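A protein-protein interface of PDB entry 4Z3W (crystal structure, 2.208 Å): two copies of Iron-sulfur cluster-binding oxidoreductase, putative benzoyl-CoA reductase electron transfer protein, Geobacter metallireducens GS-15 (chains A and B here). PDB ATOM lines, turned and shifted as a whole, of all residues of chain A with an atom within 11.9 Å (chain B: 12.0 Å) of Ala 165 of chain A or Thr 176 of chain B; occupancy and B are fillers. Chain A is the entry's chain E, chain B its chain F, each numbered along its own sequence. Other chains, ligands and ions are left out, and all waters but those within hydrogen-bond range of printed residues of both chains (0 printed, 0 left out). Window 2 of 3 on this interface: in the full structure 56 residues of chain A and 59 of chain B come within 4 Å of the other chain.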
ATOM      1  N   MET A 152       6.183 -14.941 -32.320  1.00  0.00           N
ATOM      2  CA  MET A 152       6.760 -15.589 -31.146  1.00  0.00           C
ATOM      3  C   MET A 152       8.251 -15.863 -31.326  1.00  0.00           C
ATOM      4  O   MET A 152       9.059 -15.591 -30.430  1.00  0.00           O
ATOM      5  CB  MET A 152       6.039 -16.901 -30.840  1.00  0.00           C
ATOM      6  CG  MET A 152       6.491 -17.529 -29.531  1.00  0.00           C
ATOM      7  SD  MET A 152       6.395 -19.323 -29.529  1.00  0.00           S
ATOM      8  CE  MET A 152       7.359 -19.693 -30.990  1.00  0.00           C
ATOM      9  N   GLU A 153       8.604 -16.406 -32.487  1.00  0.00           N
ATOM     10  CA  GLU A 153       9.996 -16.712 -32.821  1.00  0.00           C
ATOM     11  C   GLU A 153      10.830 -15.425 -32.877  1.00  0.00           C
ATOM     12  O   GLU A 153      11.943 -15.371 -32.357  1.00  0.00           O
ATOM     13  CB  GLU A 153      10.081 -17.472 -34.158  1.00  0.00           C
ATOM     14  CG  GLU A 153      11.104 -18.591 -34.170  1.00  0.00           C
ATOM     15  CD  GLU A 153      11.368 -19.163 -35.576  1.00  0.00           C
ATOM     16  OE1 GLU A 153      10.389 -19.483 -36.295  1.00  0.00           O
ATOM     17  OE2 GLU A 153      12.559 -19.287 -35.957  1.00  0.00           O
ATOM     18  N   GLY A 155      10.234 -12.709 -31.368  1.00  0.00           N
ATOM     19  CA  GLY A 155      10.304 -12.180 -30.021  1.00  0.00           C
ATOM     20  C   GLY A 155      11.361 -12.871 -29.181  1.00  0.00           C
ATOM     21  O   GLY A 155      12.159 -12.220 -28.508  1.00  0.00           O
ATOM     22  N   LEU A 156      11.354 -14.196 -29.198  1.00  0.00           N
ATOM     23  CA  LEU A 156      12.366 -14.955 -28.482  1.00  0.00           C
ATOM     24  C   LEU A 156      13.778 -14.678 -29.029  1.00  0.00           C
ATOM     25  O   LEU A 156      14.746 -14.642 -28.272  1.00  0.00           O
ATOM     26  CB  LEU A 156      12.042 -16.449 -28.543  1.00  0.00           C
ATOM     27  CG  LEU A 156      10.806 -16.831 -27.718  1.00  0.00           C
ATOM     28  CD1 LEU A 156      10.397 -18.279 -27.971  1.00  0.00           C
ATOM     29  CD2 LEU A 156      11.050 -16.591 -26.232  1.00  0.00           C
ATOM     30  N   GLU A 157      13.898 -14.452 -30.335  1.00  0.00           N
ATOM     31  CA  GLU A 157      15.196 -14.114 -30.916  1.00  0.00           C
ATOM     32  C   GLU A 157      15.659 -12.730 -30.464  1.00  0.00           C
ATOM     33  O   GLU A 157      16.848 -12.494 -30.288  1.00  0.00           O
ATOM     34  CB  GLU A 157      15.138 -14.197 -32.437  1.00  0.00           C
ATOM     35  CG  GLU A 157      15.276 -15.626 -32.967  1.00  0.00           C
ATOM     36  CD  GLU A 157      15.044 -15.733 -34.466  1.00  0.00           C
ATOM     37  OE1 GLU A 157      14.763 -14.691 -35.100  1.00  0.00           O
ATOM     38  OE2 GLU A 157      15.141 -16.860 -35.008  1.00  0.00           O
ATOM     39  N   SER A 158      14.714 -11.823 -30.257  1.00  0.00           N
ATOM     40  CA  SER A 158      15.012 -10.482 -29.765  1.00  0.00           C
ATOM     41  C   SER A 158      15.547 -10.523 -28.326  1.00  0.00           C
ATOM     42  O   SER A 158      16.471  -9.799 -27.982  1.00  0.00           O
ATOM     43  CB  SER A 158      13.750  -9.600 -29.847  1.00  0.00           C
ATOM     44  OG  SER A 158      13.811  -8.497 -28.956  1.00  0.00           O
ATOM     45  N   LEU A 159      14.949 -11.379 -27.501  1.00  0.00           N
ATOM     46  CA  LEU A 159      15.314 -11.531 -26.094  1.00  0.00           C
ATOM     47  C   LEU A 159      16.660 -12.242 -25.930  1.00  0.00           C
ATOM     48  O   LEU A 159      17.378 -12.010 -24.953  1.00  0.00           O
ATOM     49  CB  LEU A 159      14.232 -12.308 -25.340  1.00  0.00           C
ATOM     50  CG  LEU A 159      12.904 -11.610 -25.018  1.00  0.00           C
ATOM     51  CD1 LEU A 159      11.861 -12.618 -24.574  1.00  0.00           C
ATOM     52  CD2 LEU A 159      13.102 -10.563 -23.939  1.00  0.00           C
ATOM     53  N   ILE A 160      16.985 -13.128 -26.865  1.00  0.00           N
ATOM     54  CA  ILE A 160      18.278 -13.808 -26.824  1.00  0.00           C
ATOM     55  C   ILE A 160      19.350 -12.785 -27.168  1.00  0.00           C
ATOM     56  O   ILE A 160      20.346 -12.644 -26.468  1.00  0.00           O
ATOM     57  CB  ILE A 160      18.320 -15.008 -27.783  1.00  0.00           C
ATOM     58  CG1 ILE A 160      17.450 -16.131 -27.227  1.00  0.00           C
ATOM     59  CG2 ILE A 160      19.745 -15.503 -27.985  1.00  0.00           C
ATOM     60  CD1 ILE A 160      17.039 -17.135 -28.255  1.00  0.00           C
ATOM     61  N   SER A 161      19.099 -12.024 -28.223  1.00  0.00           N
ATOM     62  CA  SER A 161      20.006 -10.971 -28.640  1.00  0.00           C
ATOM     63  C   SER A 161      20.195  -9.879 -27.577  1.00  0.00           C
ATOM     64  O   SER A 161      21.295  -9.354 -27.431  1.00  0.00           O
ATOM     65  CB  SER A 161      19.510 -10.354 -29.946  1.00  0.00           C
ATOM     66  OG  SER A 161      20.293  -9.231 -30.292  1.00  0.00           O
ATOM     67  N   ARG A 162      19.140  -9.533 -26.832  1.00  0.00           N
ATOM     68  CA  ARG A 162      19.266  -8.491 -25.800  1.00  0.00           C
ATOM     69  C   ARG A 162      19.838  -9.011 -24.473  1.00  0.00           C
ATOM     70  O   ARG A 162      20.514  -8.266 -23.760  1.00  0.00           O
ATOM     71  CB  ARG A 162      17.918  -7.801 -25.531  1.00  0.00           C
ATOM     72  CG  ARG A 162      18.013  -6.659 -24.496  1.00  0.00           C
ATOM     73  CD  ARG A 162      16.734  -5.798 -24.399  1.00  0.00           C
ATOM     74  NE  ARG A 162      16.379  -5.197 -25.688  1.00  0.00           N
ATOM     75  CZ  ARG A 162      16.958  -4.115 -26.204  1.00  0.00           C
ATOM     76  NH1 ARG A 162      17.928  -3.491 -25.543  1.00  0.00           N
ATOM     77  NH2 ARG A 162      16.566  -3.652 -27.387  1.00  0.00           N
ATOM     78  N   PHE A 163      19.583 -10.277 -24.141  1.00  0.00           N
ATOM     79  CA  PHE A 163      19.976 -10.799 -22.826  1.00  0.00           C
ATOM     80  C   PHE A 163      20.823 -12.064 -22.869  1.00  0.00           C
ATOM     81  O   PHE A 163      21.293 -12.532 -21.832  1.00  0.00           O
ATOM     82  CB  PHE A 163      18.737 -11.070 -21.974  1.00  0.00           C
ATOM     83  CG  PHE A 163      17.894  -9.861 -21.743  1.00  0.00           C
ATOM     84  CD1 PHE A 163      18.360  -8.819 -20.960  1.00  0.00           C
ATOM     85  CD2 PHE A 163      16.639  -9.762 -22.308  1.00  0.00           C
ATOM     86  CE1 PHE A 163      17.584  -7.693 -20.738  1.00  0.00           C
ATOM     87  CE2 PHE A 163      15.852  -8.636 -22.092  1.00  0.00           C
ATOM     88  CZ  PHE A 163      16.330  -7.600 -21.301  1.00  0.00           C
ATOM     89  N   GLY A 164      21.013 -12.622 -24.057  1.00  0.00           N
ATOM     90  CA  GLY A 164      21.882 -13.782 -24.203  1.00  0.00           C
ATOM     91  C   GLY A 164      21.137 -15.094 -24.052  1.00  0.00           C
ATOM     92  O   GLY A 164      20.166 -15.196 -23.288  1.00  0.00           O
ATOM     93  N   ALA A 165      21.611 -16.101 -24.781  1.00  0.00           N
ATOM     94  CA  ALA A 165      20.932 -17.389 -24.916  1.00  0.00           C
ATOM     95  C   ALA A 165      20.900 -18.207 -23.630  1.00  0.00           C
ATOM     96  O   ALA A 165      19.901 -18.873 -23.335  1.00  0.00           O
ATOM     97  CB  ALA A 165      21.593 -18.199 -26.020  1.00  0.00           C
ATOM     98  N   ASP A 166      21.993 -18.182 -22.872  1.00  0.00           N
ATOM     99  CA  ASP A 166      22.054 -18.959 -21.632  1.00  0.00           C
ATOM    100  C   ASP A 166      21.147 -18.324 -20.574  1.00  0.00           C
ATOM    101  O   ASP A 166      20.433 -19.022 -19.847  1.00  0.00           O
ATOM    102  CB  ASP A 166      23.498 -19.071 -21.121  1.00  0.00           C
ATOM    103  N   VAL A 167      21.173 -16.997 -20.507  1.00  0.00           N
ATOM    104  CA  VAL A 167      20.345 -16.261 -19.567  1.00  0.00           C
ATOM    105  C   VAL A 167      18.857 -16.514 -19.850  1.00  0.00           C
ATOM    106  O   VAL A 167      18.064 -16.689 -18.919  1.00  0.00           O
ATOM    107  CB  VAL A 167      20.642 -14.746 -19.621  1.00  0.00           C
ATOM    108  N   VAL A 168      18.490 -16.556 -21.132  1.00  0.00           N
ATOM    109  CA  VAL A 168      17.105 -16.803 -21.537  1.00  0.00           C
ATOM    110  C   VAL A 168      16.680 -18.248 -21.289  1.00  0.00           C
ATOM    111  O   VAL A 168      15.591 -18.493 -20.774  1.00  0.00           O
ATOM    112  CB  VAL A 168      16.878 -16.481 -23.028  1.00  0.00           C
ATOM    113  CG1 VAL A 168      15.496 -16.934 -23.463  1.00  0.00           C
ATOM    114  CG2 VAL A 168      17.064 -14.999 -23.288  1.00  0.00           C
ATOM    115  N   ALA A 169      17.532 -19.200 -21.660  1.00  0.00           N
ATOM    116  CA  ALA A 169      17.209 -20.614 -21.506  1.00  0.00           C
ATOM    117  C   ALA A 169      16.926 -20.958 -20.047  1.00  0.00           C
ATOM    118  O   ALA A 169      15.920 -21.600 -19.738  1.00  0.00           O
ATOM    119  CB  ALA A 169      18.338 -21.478 -22.046  1.00  0.00           C
ATOM    120  N   ASP A 170      17.807 -20.518 -19.151  1.00  0.00           N
ATOM    121  CA  ASP A 170      17.641 -20.780 -17.719  1.00  0.00           C
ATOM    122  C   ASP A 170      16.335 -20.196 -17.163  1.00  0.00           C
ATOM    123  O   ASP A 170      15.700 -20.796 -16.295  1.00  0.00           O
ATOM    124  CB  ASP A 170      18.836 -20.228 -16.931  1.00  0.00           C
ATOM    125  N   THR A 171      15.934 -19.033 -17.667  1.00  0.00           N
ATOM    126  CA  THR A 171      14.718 -18.373 -17.193  1.00  0.00           C
ATOM    127  C   THR A 171      13.457 -19.130 -17.588  1.00  0.00           C
ATOM    128  O   THR A 171      12.613 -19.424 -16.743  1.00  0.00           O
ATOM    129  CB  THR A 171      14.614 -16.939 -17.727  1.00  0.00           C
ATOM    130  OG1 THR A 171      15.708 -16.163 -17.226  1.00  0.00           O
ATOM    131  CG2 THR A 171      13.290 -16.289 -17.290  1.00  0.00           C
ATOM    132  N   VAL A 172      13.339 -19.435 -18.878  1.00  0.00           N
ATOM    133  CA  VAL A 172      12.200 -20.178 -19.417  1.00  0.00           C
ATOM    134  C   VAL A 172      11.926 -21.449 -18.603  1.00  0.00           C
ATOM    135  O   VAL A 172      10.771 -21.852 -18.429  1.00  0.00           O
ATOM    136  CB  VAL A 172      12.427 -20.534 -20.905  1.00  0.00           C
ATOM    137  CG1 VAL A 172      11.614 -21.752 -21.307  1.00  0.00           C
ATOM    138  CG2 VAL A 172      12.093 -19.345 -21.788  1.00  0.00           C
ATOM    139  N   GLU A 173      12.987 -22.066 -18.092  1.00  0.00           N
ATOM    140  CA  GLU A 173      12.834 -23.136 -17.113  1.00  0.00           C
ATOM    141  C   GLU A 173      12.486 -22.528 -15.747  1.00  0.00           C
ATOM    142  O   GLU A 173      13.318 -22.480 -14.837  1.00  0.00           O
ATOM    143  CB  GLU A 173      14.103 -23.992 -17.028  1.00  0.00           C
ATOM    144  CG  GLU A 173      14.467 -24.732 -18.321  1.00  0.00           C
ATOM    145  CD  GLU A 173      13.680 -26.026 -18.528  1.00  0.00           C
ATOM    146  OE1 GLU A 173      13.692 -26.893 -17.623  1.00  0.00           O
ATOM    147  OE2 GLU A 173      13.056 -26.178 -19.602  1.00  0.00           O
ATOM    148  N   MET B  36      20.009  -2.962 -31.422  1.00  0.00           N
ATOM    149  CA  MET B  36      21.114  -3.849 -31.045  1.00  0.00           C
ATOM    150  C   MET B  36      22.040  -4.149 -32.221  1.00  0.00           C
ATOM    151  O   MET B  36      21.618  -4.783 -33.179  1.00  0.00           O
ATOM    152  CB  MET B  36      20.565  -5.155 -30.468  1.00  0.00           C
ATOM    153  CG  MET B  36      19.837  -4.945 -29.134  1.00  0.00           C
ATOM    154  SD  MET B  36      18.769  -6.330 -28.643  1.00  0.00           S
ATOM    155  CE  MET B  36      17.591  -6.388 -29.998  1.00  0.00           C
ATOM    156  N   MET B 152      13.391  -8.764 -18.878  1.00  0.00           N
ATOM    157  CA  MET B 152      13.555 -10.102 -19.399  1.00  0.00           C
ATOM    158  C   MET B 152      12.446 -11.035 -18.945  1.00  0.00           C
ATOM    159  O   MET B 152      11.917 -11.830 -19.726  1.00  0.00           O
ATOM    160  CB  MET B 152      14.882 -10.667 -18.960  1.00  0.00           C
ATOM    161  CG  MET B 152      14.846 -12.150 -18.935  1.00  0.00           C
ATOM    162  SD  MET B 152      15.708 -12.797 -20.362  1.00  0.00           S
ATOM    163  CE  MET B 152      16.630 -14.036 -19.494  1.00  0.00           C
ATOM    164  N   LEU B 156       9.317 -12.568 -21.385  1.00  0.00           N
ATOM    165  CA  LEU B 156       9.067 -13.989 -21.542  1.00  0.00           C
ATOM    166  C   LEU B 156       7.682 -14.390 -21.087  1.00  0.00           C
ATOM    167  O   LEU B 156       7.014 -15.181 -21.761  1.00  0.00           O
ATOM    168  CB  LEU B 156      10.126 -14.790 -20.792  1.00  0.00           C
ATOM    169  CG  LEU B 156      11.402 -14.946 -21.612  1.00  0.00           C
ATOM    170  CD1 LEU B 156      12.549 -15.359 -20.720  1.00  0.00           C
ATOM    171  CD2 LEU B 156      11.172 -15.967 -22.720  1.00  0.00           C
ATOM    172  N   VAL B 167       4.991 -24.556 -25.811  1.00  0.00           N
ATOM    173  CA  VAL B 167       5.393 -23.970 -27.088  1.00  0.00           C
ATOM    174  C   VAL B 167       6.652 -23.115 -26.936  1.00  0.00           C
ATOM    175  O   VAL B 167       7.620 -23.280 -27.686  1.00  0.00           O
ATOM    176  CB  VAL B 167       4.261 -23.101 -27.690  1.00  0.00           C
ATOM    177  CG1 VAL B 167       4.716 -22.435 -28.984  1.00  0.00           C
ATOM    178  CG2 VAL B 167       3.017 -23.937 -27.924  1.00  0.00           C
ATOM    179  N   VAL B 168       6.644 -22.215 -25.956  1.00  0.00           N
ATOM    180  CA  VAL B 168       7.763 -21.291 -25.776  1.00  0.00           C
ATOM    181  C   VAL B 168       9.050 -22.008 -25.356  1.00  0.00           C
ATOM    182  O   VAL B 168      10.125 -21.673 -25.840  1.00  0.00           O
ATOM    183  CB  VAL B 168       7.441 -20.205 -24.743  1.00  0.00           C
ATOM    184  CG1 VAL B 168       8.688 -19.398 -24.430  1.00  0.00           C
ATOM    185  CG2 VAL B 168       6.322 -19.295 -25.255  1.00  0.00           C
ATOM    186  N   ALA B 169       8.942 -22.985 -24.462  1.00  0.00           N
ATOM    187  CA  ALA B 169      10.114 -23.737 -24.027  1.00  0.00           C
ATOM    188  C   ALA B 169      10.715 -24.519 -25.202  1.00  0.00           C
ATOM    189  O   ALA B 169      11.929 -24.476 -25.433  1.00  0.00           O
ATOM    190  CB  ALA B 169       9.755 -24.681 -22.877  1.00  0.00           C
ATOM    191  N   ASP B 170       9.860 -25.229 -25.936  1.00  0.00           N
ATOM    192  CA  ASP B 170      10.293 -26.016 -27.092  1.00  0.00           C
ATOM    193  C   ASP B 170      11.047 -25.158 -28.103  1.00  0.00           C
ATOM    194  O   ASP B 170      12.093 -25.557 -28.625  1.00  0.00           O
ATOM    195  CB  ASP B 170       9.098 -26.678 -27.785  1.00  0.00           C
ATOM    196  CG  ASP B 170       8.406 -27.710 -26.909  1.00  0.00           C
ATOM    197  OD1 ASP B 170       8.926 -27.997 -25.807  1.00  0.00           O
ATOM    198  OD2 ASP B 170       7.348 -28.235 -27.331  1.00  0.00           O
ATOM    199  N   THR B 171      10.505 -23.977 -28.372  1.00  0.00           N
ATOM    200  CA  THR B 171      11.109 -23.058 -29.321  1.00  0.00           C
ATOM    201  C   THR B 171      12.446 -22.535 -28.794  1.00  0.00           C
ATOM    202  O   THR B 171      13.415 -22.415 -29.550  1.00  0.00           O
ATOM    203  CB  THR B 171      10.167 -21.877 -29.629  1.00  0.00           C
ATOM    204  OG1 THR B 171       8.917 -22.375 -30.123  1.00  0.00           O
ATOM    205  CG2 THR B 171      10.786 -20.950 -30.667  1.00  0.00           C
ATOM    206  N   VAL B 172      12.496 -22.232 -27.497  1.00  0.00           N
ATOM    207  CA  VAL B 172      13.722 -21.744 -26.869  1.00  0.00           C
ATOM    208  C   VAL B 172      14.804 -22.822 -26.901  1.00  0.00           C
ATOM    209  O   VAL B 172      15.976 -22.537 -27.150  1.00  0.00           O
ATOM    210  CB  VAL B 172      13.479 -21.300 -25.410  1.00  0.00           C
ATOM    211  CG1 VAL B 172      14.809 -21.106 -24.680  1.00  0.00           C
ATOM    212  CG2 VAL B 172      12.652 -20.018 -25.371  1.00  0.00           C
ATOM    213  N   GLU B 173      14.392 -24.058 -26.642  1.00  0.00           N
ATOM    214  CA  GLU B 173      15.265 -25.217 -26.746  1.00  0.00           C
ATOM    215  C   GLU B 173      15.932 -25.277 -28.117  1.00  0.00           C
ATOM    216  O   GLU B 173      17.150 -25.421 -28.227  1.00  0.00           O
ATOM    217  CB  GLU B 173      14.464 -26.500 -26.489  1.00  0.00           C
ATOM    218  CG  GLU B 173      15.185 -27.803 -26.847  1.00  0.00           C
ATOM    219  CD  GLU B 173      16.034 -28.343 -25.708  1.00  0.00           C
ATOM    220  OE1 GLU B 173      16.272 -27.596 -24.735  1.00  0.00           O
ATOM    221  OE2 GLU B 173      16.455 -29.518 -25.783  1.00  0.00           O
ATOM    222  N   GLN B 174      15.122 -25.146 -29.161  1.00  0.00           N
ATOM    223  CA  GLN B 174      15.595 -25.310 -30.530  1.00  0.00           C
ATOM    224  C   GLN B 174      16.421 -24.140 -31.030  1.00  0.00           C
ATOM    225  O   GLN B 174      16.892 -24.149 -32.161  1.00  0.00           O
ATOM    226  CB  GLN B 174      14.414 -25.521 -31.465  1.00  0.00           C
ATOM    227  CG  GLN B 174      13.779 -26.877 -31.322  1.00  0.00           C
ATOM    228  CD  GLN B 174      12.846 -27.182 -32.467  1.00  0.00           C
ATOM    229  OE1 GLN B 174      11.935 -26.401 -32.762  1.00  0.00           O
ATOM    230  NE2 GLN B 174      13.077 -28.313 -33.138  1.00  0.00           N
ATOM    231  N   LEU B 175      16.593 -23.132 -30.186  1.00  0.00           N
ATOM    232  CA  LEU B 175      17.314 -21.929 -30.571  1.00  0.00           C
ATOM    233  C   LEU B 175      18.630 -21.803 -29.810  1.00  0.00           C
ATOM    234  O   LEU B 175      19.461 -20.952 -30.130  1.00  0.00           O
ATOM    235  CB  LEU B 175      16.437 -20.694 -30.331  1.00  0.00           C
ATOM    236  CG  LEU B 175      15.491 -20.273 -31.457  1.00  0.00           C
ATOM    237  CD1 LEU B 175      14.196 -19.712 -30.886  1.00  0.00           C
ATOM    238  CD2 LEU B 175      16.169 -19.237 -32.347  1.00  0.00           C
ATOM    239  N   THR B 176      18.812 -22.657 -28.805  1.00  0.00           N
ATOM    240  CA  THR B 176      19.987 -22.601 -27.938  1.00  0.00           C
ATOM    241  C   THR B 176      20.689 -23.953 -27.848  1.00  0.00           C
ATOM    242  O   THR B 176      21.071 -24.535 -28.863  1.00  0.00           O
ATOM    243  CB  THR B 176      19.610 -22.136 -26.514  1.00  0.00           C
ATOM    244  OG1 THR B 176      18.767 -23.116 -25.892  1.00  0.00           O
ATOM    245  CG2 THR B 176      18.879 -20.801 -26.558  1.00  0.00           C
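OG of Ser 161 of chain A is in hydrogen-bond range of SD of Met 36 of chain B, 3.7 Å away. The guanidinium group of Arg 162 of chain A sits close to the side-chain sulfur of Met 36 of chain B.
Among the printed residues, pairs that only touch across the chains: Val 167 of chain A with Met 152 of chain B, Met 152 of chain A with Thr 171 of chain B, Thr 171 of chain A with Met 152 of chain B, Val 168 of chain A with Met 152 of chain B, Leu 156 of chain A with Leu 156 of chain B, Met 152 of chain A with Val 167 of chain B, Val 172 of chain A with Leu 156 of chain B, Thr 171 of chain A with Leu 156 of chain B, Val 172 of chain A with Ala 169 of chain B, Val 172 of chain A with Val 172 of chain B, Glu 157 of chain A with Leu 175 of chain B, Phe 163 of chain A with Met 152 of chain B, Leu 159 of chain A with Leu 156 of chain B, Ala 165 of chain A with Thr 176 of chain B, Leu 156 of chain A with Thr 171 of chain B and Leu 156 of chain A with Val 172 of chain B.
Hydrophobic or aromatic side chains of chain B that line the printed part of chain A: Met 36, Met 152, Leu 156, Val 167, Ala 169, Val 172 and Leu 175. Of the 21 printed residues of chain A, 12 touch a printed residue of chain B. Hydrophobic or aromatic side chains of chain A within 4 Å of the printed part of chain B: Met 152, Leu 156, Leu 159, Phe 163, Ala 165, Val 168 and Val 172. Among the printed residues, no Asp or Glu carboxylate lies within 4 Å of a Lys or Arg side-chain nitrogen of the other chain.
O of Val 167 of chain A sits at hydrogen-bond distance from OG1 of Thr 171 of chain A (2.9 Å). O of Val 167 of chain B sits at hydrogen-bond distance from OG1 of Thr 171 of chain B. OG1 of Thr 176 of chain B lies within hydrogen-bond range of O of Val 172 of chain B, 3.1 Å away.
Ala 165 of chain A touches just one residue of chain B: Thr 176. Of the printed residues of chain A, Thr 176 of chain B touches Ala 165. No residue of chain B comes within 4 Å of Ile 160 of chain A. Val 168 of chain A touches one residue of chain B. No residue of chain A comes within 4 Å of Glu 173 of chain B. Of the printed residues of chain B, Arg 162 of chain A touches Met 36 (3.5 Å). Of the printed residues of chain A, Val 172 of chain B touches Leu 156 (3.9 Å) and Val 172 (3.7 Å). Printed residues of chain B within 4 Å of Phe 163 of chain A: Met 152 (3.7 Å). Gln 174 of chain B touches none of the printed residues of chain A. Glu 153 of chain A touches none of the printed residues of chain B. The nearest printed residue of chain B that does not touch Met 152 of chain A is Val 168 of chain B (4.3 Å).
Leu 156 of chain B touches its own counterpart, Leu 156 of chain A. Leu 156 of chain A touches Val 172 of chain B, and with the chains exchanged Val 172 of chain A touches Leu 156 of chain B. Val 172 of chain A touches Ala 169 of chain B, but with the chains exchanged Ala 169 of chain A does not touch Val 172 of chain B (4.01 Å). Val 172 of chain B touches its own counterpart, Val 172 of chain A. 9 positions are printed for both chains. Of the 18 pairs that touch across the chains among the printed residues, 10 have their exchanged pair printed and touching as well.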
